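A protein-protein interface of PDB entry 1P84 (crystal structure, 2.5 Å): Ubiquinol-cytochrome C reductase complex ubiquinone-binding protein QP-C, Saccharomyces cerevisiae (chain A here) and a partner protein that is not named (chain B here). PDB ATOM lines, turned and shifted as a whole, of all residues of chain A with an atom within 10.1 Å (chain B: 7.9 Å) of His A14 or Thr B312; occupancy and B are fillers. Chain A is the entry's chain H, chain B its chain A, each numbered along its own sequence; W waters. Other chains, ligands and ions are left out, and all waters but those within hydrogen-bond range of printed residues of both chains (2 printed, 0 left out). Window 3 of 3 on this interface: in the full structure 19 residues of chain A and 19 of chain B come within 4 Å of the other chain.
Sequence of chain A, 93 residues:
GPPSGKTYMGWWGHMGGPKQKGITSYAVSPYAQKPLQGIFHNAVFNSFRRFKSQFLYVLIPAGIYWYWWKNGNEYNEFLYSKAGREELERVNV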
ATOM      1  N   SER A   4     -18.634 -15.472 -23.208  1.00  0.00           N
ATOM      2  CA  SER A   4     -18.859 -16.720 -23.933  1.00  0.00           C
ATOM      3  C   SER A   4     -19.124 -17.945 -23.036  1.00  0.00           C
ATOM      4  O   SER A   4     -18.549 -18.070 -21.949  1.00  0.00           O
ATOM      5  CB  SER A   4     -17.657 -16.991 -24.848  1.00  0.00           C
ATOM      6  OG  SER A   4     -17.837 -18.170 -25.617  1.00  0.00           O
ATOM      7  N   LYS A   6     -19.090 -21.807 -21.573  1.00  0.00           N
ATOM      8  CA  LYS A   6     -18.012 -22.777 -21.345  1.00  0.00           C
ATOM      9  C   LYS A   6     -18.142 -23.974 -22.282  1.00  0.00           C
ATOM     10  O   LYS A   6     -19.232 -24.524 -22.460  1.00  0.00           O
ATOM     11  CB  LYS A   6     -17.986 -23.247 -19.881  1.00  0.00           C
ATOM     12  CG  LYS A   6     -17.515 -22.191 -18.880  1.00  0.00           C
ATOM     13  CD  LYS A   6     -16.044 -21.837 -19.077  1.00  0.00           C
ATOM     14  CE  LYS A   6     -15.671 -20.503 -18.404  1.00  0.00           C
ATOM     15  NZ  LYS A   6     -15.801 -20.504 -16.914  1.00  0.00           N
ATOM     16  N   THR A   7     -17.017 -24.367 -22.871  1.00  0.00           N
ATOM     17  CA  THR A   7     -16.972 -25.480 -23.811  1.00  0.00           C
ATOM     18  C   THR A   7     -15.977 -26.548 -23.358  1.00  0.00           C
ATOM     19  O   THR A   7     -15.454 -26.483 -22.243  1.00  0.00           O
ATOM     20  CB  THR A   7     -16.569 -24.984 -25.220  1.00  0.00           C
ATOM     21  OG1 THR A   7     -15.320 -24.281 -25.152  1.00  0.00           O
ATOM     22  CG2 THR A   7     -17.630 -24.052 -25.780  1.00  0.00           C
ATOM     23  N   TYR A   8     -15.743 -27.545 -24.208  1.00  0.00           N
ATOM     24  CA  TYR A   8     -14.788 -28.605 -23.885  1.00  0.00           C
ATOM     25  C   TYR A   8     -13.559 -28.514 -24.783  1.00  0.00           C
ATOM     26  O   TYR A   8     -12.807 -29.478 -24.934  1.00  0.00           O
ATOM     27  CB  TYR A   8     -15.440 -29.992 -23.971  1.00  0.00           C
ATOM     28  CG  TYR A   8     -16.458 -30.239 -22.878  1.00  0.00           C
ATOM     29  CD1 TYR A   8     -17.817 -30.038 -23.110  1.00  0.00           C
ATOM     30  CD2 TYR A   8     -16.056 -30.614 -21.594  1.00  0.00           C
ATOM     31  CE1 TYR A   8     -18.754 -30.196 -22.097  1.00  0.00           C
ATOM     32  CE2 TYR A   8     -16.984 -30.774 -20.572  1.00  0.00           C
ATOM     33  CZ  TYR A   8     -18.337 -30.560 -20.833  1.00  0.00           C
ATOM     34  OH  TYR A   8     -19.272 -30.686 -19.828  1.00  0.00           O
ATOM     35  N   MET A   9     -13.389 -27.355 -25.414  1.00  0.00           N
ATOM     36  CA  MET A   9     -12.238 -27.097 -26.271  1.00  0.00           C
ATOM     37  C   MET A   9     -11.860 -25.628 -26.175  1.00  0.00           C
ATOM     38  O   MET A   9     -12.723 -24.756 -26.204  1.00  0.00           O
ATOM     39  CB  MET A   9     -12.502 -27.462 -27.736  1.00  0.00           C
ATOM     40  CG  MET A   9     -11.244 -27.308 -28.581  1.00  0.00           C
ATOM     41  SD  MET A   9     -11.407 -27.580 -30.346  1.00  0.00           S
ATOM     42  CE  MET A   9     -12.165 -26.029 -30.873  1.00  0.00           C
ATOM     43  N   GLY A  10     -10.567 -25.369 -26.016  1.00  0.00           N
ATOM     44  CA  GLY A  10     -10.081 -24.003 -25.932  1.00  0.00           C
ATOM     45  C   GLY A  10      -9.330 -23.660 -27.203  1.00  0.00           C
ATOM     46  O   GLY A  10      -9.797 -23.953 -28.308  1.00  0.00           O
ATOM     47  N   TRP A  11      -8.146 -23.076 -27.049  1.00  0.00           N
ATOM     48  CA  TRP A  11      -7.316 -22.700 -28.196  1.00  0.00           C
ATOM     49  C   TRP A  11      -5.852 -22.839 -27.771  1.00  0.00           C
ATOM     50  O   TRP A  11      -5.577 -23.051 -26.600  1.00  0.00           O
ATOM     51  CB  TRP A  11      -7.625 -21.252 -28.624  1.00  0.00           C
ATOM     52  CG  TRP A  11      -7.344 -20.964 -30.085  1.00  0.00           C
ATOM     53  CD1 TRP A  11      -6.272 -20.281 -30.601  1.00  0.00           C
ATOM     54  CD2 TRP A  11      -8.146 -21.350 -31.208  1.00  0.00           C
ATOM     55  NE1 TRP A  11      -6.362 -20.219 -31.968  1.00  0.00           N
ATOM     56  CE2 TRP A  11      -7.500 -20.866 -32.369  1.00  0.00           C
ATOM     57  CE3 TRP A  11      -9.346 -22.058 -31.349  1.00  0.00           C
ATOM     58  CZ2 TRP A  11      -8.017 -21.066 -33.652  1.00  0.00           C
ATOM     59  CZ3 TRP A  11      -9.859 -22.252 -32.628  1.00  0.00           C
ATOM     60  CH2 TRP A  11      -9.193 -21.760 -33.758  1.00  0.00           C
ATOM     61  N   TRP A  12      -4.930 -22.754 -28.724  1.00  0.00           N
ATOM     62  CA  TRP A  12      -3.500 -22.864 -28.448  1.00  0.00           C
ATOM     63  C   TRP A  12      -3.064 -22.104 -27.187  1.00  0.00           C
ATOM     64  O   TRP A  12      -3.235 -20.883 -27.088  1.00  0.00           O
ATOM     65  CB  TRP A  12      -2.703 -22.362 -29.654  1.00  0.00           C
ATOM     66  CG  TRP A  12      -3.062 -23.067 -30.919  1.00  0.00           C
ATOM     67  CD1 TRP A  12      -3.806 -22.573 -31.947  1.00  0.00           C
ATOM     68  CD2 TRP A  12      -2.720 -24.408 -31.282  1.00  0.00           C
ATOM     69  NE1 TRP A  12      -3.952 -23.521 -32.927  1.00  0.00           N
ATOM     70  CE2 TRP A  12      -3.294 -24.659 -32.545  1.00  0.00           C
ATOM     71  CE3 TRP A  12      -1.982 -25.426 -30.663  1.00  0.00           C
ATOM     72  CZ2 TRP A  12      -3.150 -25.892 -33.207  1.00  0.00           C
ATOM     73  CZ3 TRP A  12      -1.838 -26.651 -31.317  1.00  0.00           C
ATOM     74  CH2 TRP A  12      -2.419 -26.871 -32.576  1.00  0.00           C
ATOM     75  N   GLY A  13      -2.532 -22.845 -26.215  1.00  0.00           N
ATOM     76  CA  GLY A  13      -2.090 -22.242 -24.973  1.00  0.00           C
ATOM     77  C   GLY A  13      -3.048 -22.471 -23.817  1.00  0.00           C
ATOM     78  O   GLY A  13      -2.681 -22.283 -22.663  1.00  0.00           O
ATOM     79  N   HIS A  14      -4.294 -22.806 -24.129  1.00  0.00           N
ATOM     80  CA  HIS A  14      -5.317 -23.081 -23.121  1.00  0.00           C
ATOM     81  C   HIS A  14      -6.378 -24.013 -23.722  1.00  0.00           C
ATOM     82  O   HIS A  14      -7.576 -23.776 -23.608  1.00  0.00           O
ATOM     83  CB  HIS A  14      -5.937 -21.780 -22.579  1.00  0.00           C
ATOM     84  CG  HIS A  14      -6.579 -20.910 -23.623  1.00  0.00           C
ATOM     85  ND1 HIS A  14      -7.944 -20.723 -23.699  1.00  0.00           N
ATOM     86  CD2 HIS A  14      -6.043 -20.154 -24.611  1.00  0.00           C
ATOM     87  CE1 HIS A  14      -8.222 -19.892 -24.689  1.00  0.00           C
ATOM     88  NE2 HIS A  14      -7.086 -19.532 -25.258  1.00  0.00           N
ATOM     89  N   MET A  15      -5.903 -25.099 -24.326  1.00  0.00           N
ATOM     90  CA  MET A  15      -6.747 -26.084 -24.987  1.00  0.00           C
ATOM     91  C   MET A  15      -7.776 -26.761 -24.090  1.00  0.00           C
ATOM     92  O   MET A  15      -8.803 -27.239 -24.583  1.00  0.00           O
ATOM     93  CB  MET A  15      -5.879 -27.144 -25.658  1.00  0.00           C
ATOM     94  CG  MET A  15      -6.521 -27.807 -26.855  1.00  0.00           C
ATOM     95  SD  MET A  15      -6.703 -26.653 -28.206  1.00  0.00           S
ATOM     96  CE  MET A  15      -4.979 -26.590 -28.834  1.00  0.00           C
ATOM     97  N   GLY A  16      -7.506 -26.816 -22.786  1.00  0.00           N
ATOM     98  CA  GLY A  16      -8.441 -27.438 -21.865  1.00  0.00           C
ATOM     99  C   GLY A  16      -8.061 -28.826 -21.358  1.00  0.00           C
ATOM    100  O   GLY A  16      -8.814 -29.444 -20.597  1.00  0.00           O
ATOM    101  N   GLY A  17      -6.907 -29.330 -21.783  1.00  0.00           N
ATOM    102  CA  GLY A  17      -6.469 -30.637 -21.332  1.00  0.00           C
ATOM    103  C   GLY A  17      -5.840 -30.570 -19.957  1.00  0.00           C
ATOM    104  O   GLY A  17      -5.776 -29.500 -19.357  1.00  0.00           O
ATOM    105  N   PRO A  18      -5.381 -31.700 -19.414  1.00  0.00           N
ATOM    106  CA  PRO A  18      -4.759 -31.705 -18.091  1.00  0.00           C
ATOM    107  C   PRO A  18      -3.294 -31.261 -18.201  1.00  0.00           C
ATOM    108  O   PRO A  18      -2.690 -31.350 -19.277  1.00  0.00           O
ATOM    109  CB  PRO A  18      -4.872 -33.169 -17.690  1.00  0.00           C
ATOM    110  CG  PRO A  18      -4.608 -33.864 -18.989  1.00  0.00           C
ATOM    111  CD  PRO A  18      -5.465 -33.069 -19.958  1.00  0.00           C
ATOM    112  N   LYS A  19      -2.724 -30.795 -17.092  1.00  0.00           N
ATOM    113  CA  LYS A  19      -1.335 -30.353 -17.100  1.00  0.00           C
ATOM    114  C   LYS A  19      -0.403 -31.502 -17.438  1.00  0.00           C
ATOM    115  O   LYS A  19      -0.437 -32.544 -16.798  1.00  0.00           O
ATOM    116  CB  LYS A  19      -0.957 -29.725 -15.762  1.00  0.00           C
ATOM    117  CG  LYS A  19      -1.802 -28.523 -15.409  1.00  0.00           C
ATOM    118  CD  LYS A  19      -1.184 -27.713 -14.282  1.00  0.00           C
ATOM    119  CE  LYS A  19      -2.221 -26.803 -13.626  1.00  0.00           C
ATOM    120  NZ  LYS A  19      -3.015 -26.037 -14.642  1.00  0.00           N
ATOM    121  N   GLN A  20       0.389 -31.324 -18.486  1.00  0.00           N
ATOM    122  CA  GLN A  20       1.322 -32.347 -18.935  1.00  0.00           C
ATOM    123  C   GLN A  20       2.702 -32.115 -18.344  1.00  0.00           C
ATOM    124  O   GLN A  20       3.126 -30.981 -18.190  1.00  0.00           O
ATOM    125  CB  GLN A  20       1.404 -32.342 -20.462  1.00  0.00           C
ATOM    126  CG  GLN A  20       0.070 -32.535 -21.166  1.00  0.00           C
ATOM    127  CD  GLN A  20       0.226 -32.644 -22.670  1.00  0.00           C
ATOM    128  OE1 GLN A  20       1.312 -32.949 -23.172  1.00  0.00           O
ATOM    129  NE2 GLN A  20      -0.859 -32.395 -23.402  1.00  0.00           N
ATOM    130  N   ARG B 226       7.744 -30.405 -22.934  1.00  0.00           N
ATOM    131  CA  ARG B 226       6.587 -29.754 -22.326  1.00  0.00           C
ATOM    132  C   ARG B 226       6.512 -29.990 -20.828  1.00  0.00           C
ATOM    133  O   ARG B 226       6.798 -31.079 -20.350  1.00  0.00           O
ATOM    134  CB  ARG B 226       5.280 -30.212 -22.992  1.00  0.00           C
ATOM    135  CG  ARG B 226       4.218 -29.110 -23.071  1.00  0.00           C
ATOM    136  CD  ARG B 226       2.824 -29.577 -22.668  1.00  0.00           C
ATOM    137  NE  ARG B 226       1.879 -29.627 -23.785  1.00  0.00           N
ATOM    138  CZ  ARG B 226       0.590 -29.299 -23.703  1.00  0.00           C
ATOM    139  NH1 ARG B 226      -0.177 -29.398 -24.777  1.00  0.00           N
ATOM    140  NH2 ARG B 226       0.061 -28.864 -22.567  1.00  0.00           N
ATOM    141  N   THR B 308       9.032 -16.418 -22.334  1.00  0.00           N
ATOM    142  CA  THR B 308       7.766 -15.688 -22.346  1.00  0.00           C
ATOM    143  C   THR B 308       6.703 -16.219 -21.392  1.00  0.00           C
ATOM    144  O   THR B 308       6.694 -17.386 -21.039  1.00  0.00           O
ATOM    145  CB  THR B 308       7.180 -15.672 -23.773  1.00  0.00           C
ATOM    146  OG1 THR B 308       5.894 -15.053 -23.754  1.00  0.00           O
ATOM    147  CG2 THR B 308       7.061 -17.094 -24.325  1.00  0.00           C
ATOM    148  N   ARG B 309       5.814 -15.331 -20.981  1.00  0.00           N
ATOM    149  CA  ARG B 309       4.705 -15.650 -20.089  1.00  0.00           C
ATOM    150  C   ARG B 309       3.384 -15.483 -20.859  1.00  0.00           C
ATOM    151  O   ARG B 309       2.300 -15.731 -20.324  1.00  0.00           O
ATOM    152  CB  ARG B 309       4.709 -14.704 -18.884  1.00  0.00           C
ATOM    153  CG  ARG B 309       5.666 -15.094 -17.780  1.00  0.00           C
ATOM    154  CD  ARG B 309       6.191 -13.874 -17.033  1.00  0.00           C
ATOM    155  NE  ARG B 309       5.153 -12.888 -16.742  1.00  0.00           N
ATOM    156  CZ  ARG B 309       5.213 -11.607 -17.103  1.00  0.00           C
ATOM    157  NH1 ARG B 309       4.219 -10.778 -16.800  1.00  0.00           N
ATOM    158  NH2 ARG B 309       6.265 -11.148 -17.766  1.00  0.00           N
ATOM    159  N   ASN B 310       3.484 -14.993 -22.093  1.00  0.00           N
ATOM    160  CA  ASN B 310       2.325 -14.794 -22.937  1.00  0.00           C
ATOM    161  C   ASN B 310       2.180 -16.113 -23.674  1.00  0.00           C
ATOM    162  O   ASN B 310       2.517 -16.224 -24.857  1.00  0.00           O
ATOM    163  CB  ASN B 310       2.574 -13.658 -23.925  1.00  0.00           C
ATOM    164  CG  ASN B 310       1.302 -13.185 -24.607  1.00  0.00           C
ATOM    165  OD1 ASN B 310       1.203 -12.032 -25.023  1.00  0.00           O
ATOM    166  ND2 ASN B 310       0.324 -14.073 -24.727  1.00  0.00           N
ATOM    167  N   VAL B 311       1.655 -17.109 -22.970  1.00  0.00           N
ATOM    168  CA  VAL B 311       1.512 -18.443 -23.533  1.00  0.00           C
ATOM    169  C   VAL B 311       0.434 -18.643 -24.589  1.00  0.00           C
ATOM    170  O   VAL B 311       0.338 -19.722 -25.159  1.00  0.00           O
ATOM    171  CB  VAL B 311       1.378 -19.506 -22.420  1.00  0.00           C
ATOM    172  CG1 VAL B 311       2.626 -19.491 -21.547  1.00  0.00           C
ATOM    173  CG2 VAL B 311       0.130 -19.252 -21.580  1.00  0.00           C
ATOM    174  N   THR B 312      -0.360 -17.614 -24.874  1.00  0.00           N
ATOM    175  CA  THR B 312      -1.396 -17.750 -25.892  1.00  0.00           C
ATOM    176  C   THR B 312      -1.035 -17.077 -27.209  1.00  0.00           C
ATOM    177  O   THR B 312      -1.775 -17.191 -28.183  1.00  0.00           O
ATOM    178  CB  THR B 312      -2.768 -17.233 -25.409  1.00  0.00           C
ATOM    179  OG1 THR B 312      -2.675 -15.861 -25.022  1.00  0.00           O
ATOM    180  CG2 THR B 312      -3.254 -18.043 -24.230  1.00  0.00           C
ATOM    181  N   MET B 313       0.123 -16.414 -27.249  1.00  0.00           N
ATOM    182  CA  MET B 313       0.565 -15.718 -28.462  1.00  0.00           C
ATOM    183  C   MET B 313       1.972 -16.103 -28.940  1.00  0.00           C
ATOM    184  O   MET B 313       2.610 -15.367 -29.699  1.00  0.00           O
ATOM    185  CB  MET B 313       0.459 -14.203 -28.263  1.00  0.00           C
ATOM    186  CG  MET B 313      -0.919 -13.767 -27.792  1.00  0.00           C
ATOM    187  SD  MET B 313      -1.163 -12.008 -27.738  1.00  0.00           S
ATOM    188  CE  MET B 313      -1.199 -11.663 -29.501  1.00  0.00           C
ATOM    189  N   ILE B 314       2.429 -17.282 -28.540  1.00  0.00           N
ATOM    190  CA  ILE B 314       3.749 -17.760 -28.924  1.00  0.00           C
ATOM    191  C   ILE B 314       3.903 -17.836 -30.441  1.00  0.00           C
ATOM    192  O   ILE B 314       4.992 -17.598 -30.954  1.00  0.00           O
ATOM    193  CB  ILE B 314       4.054 -19.149 -28.274  1.00  0.00           C
ATOM    194  CG1 ILE B 314       4.074 -19.026 -26.757  1.00  0.00           C
ATOM    195  CG2 ILE B 314       5.372 -19.702 -28.726  1.00  0.00           C
ATOM    196  CD1 ILE B 314       4.230 -20.348 -26.065  1.00  0.00           C
ATOM    197  N   ASP B 315       2.834 -18.140 -31.173  1.00  0.00           N
ATOM    198  CA  ASP B 315       2.971 -18.232 -32.624  1.00  0.00           C
ATOM    199  C   ASP B 315       3.312 -16.884 -33.257  1.00  0.00           C
ATOM    200  O   ASP B 315       4.035 -16.825 -34.251  1.00  0.00           O
ATOM    201  CB  ASP B 315       1.762 -18.911 -33.302  1.00  0.00           C
ATOM    202  CG  ASP B 315       0.450 -18.166 -33.102  1.00  0.00           C
ATOM    203  OD1 ASP B 315      -0.068 -18.153 -31.966  1.00  0.00           O
ATOM    204  OD2 ASP B 315      -0.095 -17.636 -34.094  1.00  0.00           O
ATOM    205  N   ASP B 316       2.832 -15.802 -32.653  1.00  0.00           N
ATOM    206  CA  ASP B 316       3.132 -14.473 -33.164  1.00  0.00           C
ATOM    207  C   ASP B 316       4.592 -14.115 -32.866  1.00  0.00           C
ATOM    208  O   ASP B 316       5.275 -13.528 -33.707  1.00  0.00           O
ATOM    209  CB  ASP B 316       2.185 -13.435 -32.573  1.00  0.00           C
ATOM    210  CG  ASP B 316       0.766 -13.567 -33.110  1.00  0.00           C
ATOM    211  OD1 ASP B 316      -0.167 -13.729 -32.294  1.00  0.00           O
ATOM    212  OD2 ASP B 316       0.584 -13.518 -34.346  1.00  0.00           O
ATOM    213  N   GLN B 412       5.411 -24.106 -20.568  1.00  0.00           N
ATOM    214  CA  GLN B 412       4.107 -24.056 -21.229  1.00  0.00           C
ATOM    215  C   GLN B 412       4.206 -23.837 -22.741  1.00  0.00           C
ATOM    216  O   GLN B 412       3.791 -22.791 -23.240  1.00  0.00           O
ATOM    217  CB  GLN B 412       3.245 -22.956 -20.596  1.00  0.00           C
ATOM    218  CG  GLN B 412       3.111 -23.065 -19.087  1.00  0.00           C
ATOM    219  CD  GLN B 412       1.956 -22.242 -18.539  1.00  0.00           C
ATOM    220  OE1 GLN B 412       2.031 -21.684 -17.443  1.00  0.00           O
ATOM    221  NE2 GLN B 412       0.869 -22.181 -19.295  1.00  0.00           N
ATOM    222  N   GLU B 414       2.546 -25.383 -25.288  1.00  0.00           N
ATOM    223  CA  GLU B 414       1.437 -25.901 -26.084  1.00  0.00           C
ATOM    224  C   GLU B 414       1.195 -24.977 -27.294  1.00  0.00           C
ATOM    225  O   GLU B 414       0.880 -25.441 -28.389  1.00  0.00           O
ATOM    226  CB  GLU B 414       0.163 -26.007 -25.240  1.00  0.00           C
ATOM    227  CG  GLU B 414      -1.079 -26.440 -26.020  1.00  0.00           C
ATOM    228  CD  GLU B 414      -2.313 -26.534 -25.138  1.00  0.00           C
ATOM    229  OE1 GLU B 414      -3.069 -25.549 -25.041  1.00  0.00           O
ATOM    230  OE2 GLU B 414      -2.536 -27.604 -24.535  1.00  0.00           O
ATOM    231  N   GLY B 415       1.392 -23.678 -27.087  1.00  0.00           N
ATOM    232  CA  GLY B 415       1.195 -22.702 -28.139  1.00  0.00           C
ATOM    233  C   GLY B 415       2.240 -22.655 -29.245  1.00  0.00           C
ATOM    234  O   GLY B 415       2.031 -21.977 -30.253  1.00  0.00           O
ATOM    235  N   LEU B 416       3.374 -23.323 -29.052  1.00  0.00           N
ATOM    236  CA  LEU B 416       4.423 -23.349 -30.068  1.00  0.00           C
ATOM    237  C   LEU B 416       3.937 -24.314 -31.142  1.00  0.00           C
ATOM    238  O   LEU B 416       3.846 -25.512 -30.908  1.00  0.00           O
ATOM    239  CB  LEU B 416       5.742 -23.836 -29.451  1.00  0.00           C
ATOM    240  CG  LEU B 416       6.969 -23.973 -30.358  1.00  0.00           C
ATOM    241  CD1 LEU B 416       7.540 -22.610 -30.714  1.00  0.00           C
ATOM    242  CD2 LEU B 416       8.014 -24.797 -29.654  1.00  0.00           C
HETATM  243  O   HOH W   1      -4.518 -18.574 -28.415  1.00  0.00           O
HETATM  244  O   HOH W   2      -4.043 -28.107 -22.142  1.00  0.00           O
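The backbone NH of His A14 is in hydrogen-bond range of the side-chain carboxylate of Glu B414 (3.1 Å).
N of Met A15 sits at hydrogen-bond distance from OE1 of Glu B414 (3.0 Å).
NE2 of Gln A20 sits close to NH1 of Arg B226, 3.4 Å away.
The side-chain carboxylate (OE1) of Glu B414 lies within hydrogen-bond range of the backbone NH (N) of Gly A13, 3.0 Å away.
The side-chain carboxylate (OE2) of Glu B414 is in salt-bridge range of the guanidinium group (NH1) of Arg B226, at 3.0 Å.
O of Met A15 is in hydrogen-bond range of N of Gly A10.
Glu B414 touches Trp A11.
Trp A12 touches Thr B312.
Trp A12 touches Glu B414 (CE3 to O, 3.7 Å).
Val B311 touches Gly A13 (O to CA, 3.5 Å).
CG2 of Thr B312 touches CD2 of His A14, 3.5 Å away.
Printed residues of chain B within 4 Å of His A14: Thr B312 and Glu B414.
Of chain A, only Trp A12 (3.8 Å) and His A14 (3.5 Å) come within 4 Å of Thr B312.
Of the printed residues of chain B, Gly A13 touches Val B311 and Glu B414.
No residue of chain A comes within 4 Å of Asn B310.
Of chain A, only Gly A13 comes within 4 Å of Val B311.
Of the printed residues of chain A, Glu B414 touches Trp A11, Trp A12, Gly A13, His A14 and Met A15.
Of the printed residues of chain B, Trp A12 touches Thr B312 and Glu B414.
Of the printed residues of chain A, Arg B226 touches Gln A20 (3.4 Å).
Of the printed residues of chain B, Trp A11 touches Glu B414 (3.9 Å).
Of the printed residues of chain B, Gln A20 touches Arg B226 (3.4 Å).
The nearest residue of chain A that does not touch Thr B312 is Gly A13 (4.4 Å).
The nearest printed residue of chain B that does not touch Gln A20 is Glu B414 (5.2 Å).
Of the 14 printed residues of chain B, 4 touch a printed residue of chain A.
Along chain B the printed residues that touch a printed residue of chain A span positions 226 to 414.
Of the 16 printed residues of chain A, 6 touch a printed residue of chain B.
Among the printed residues, 9 pairs touch across the chains.
Water W2 lies within hydrogen-bond range of OE2 of Glu B414 (2.9 Å) and N of Gly A17 (3.1 Å).
Water W1 lies within hydrogen-bond range of the backbone carbonyl oxygen of Trp A12 and the backbone carbonyl oxygen of Thr B312.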
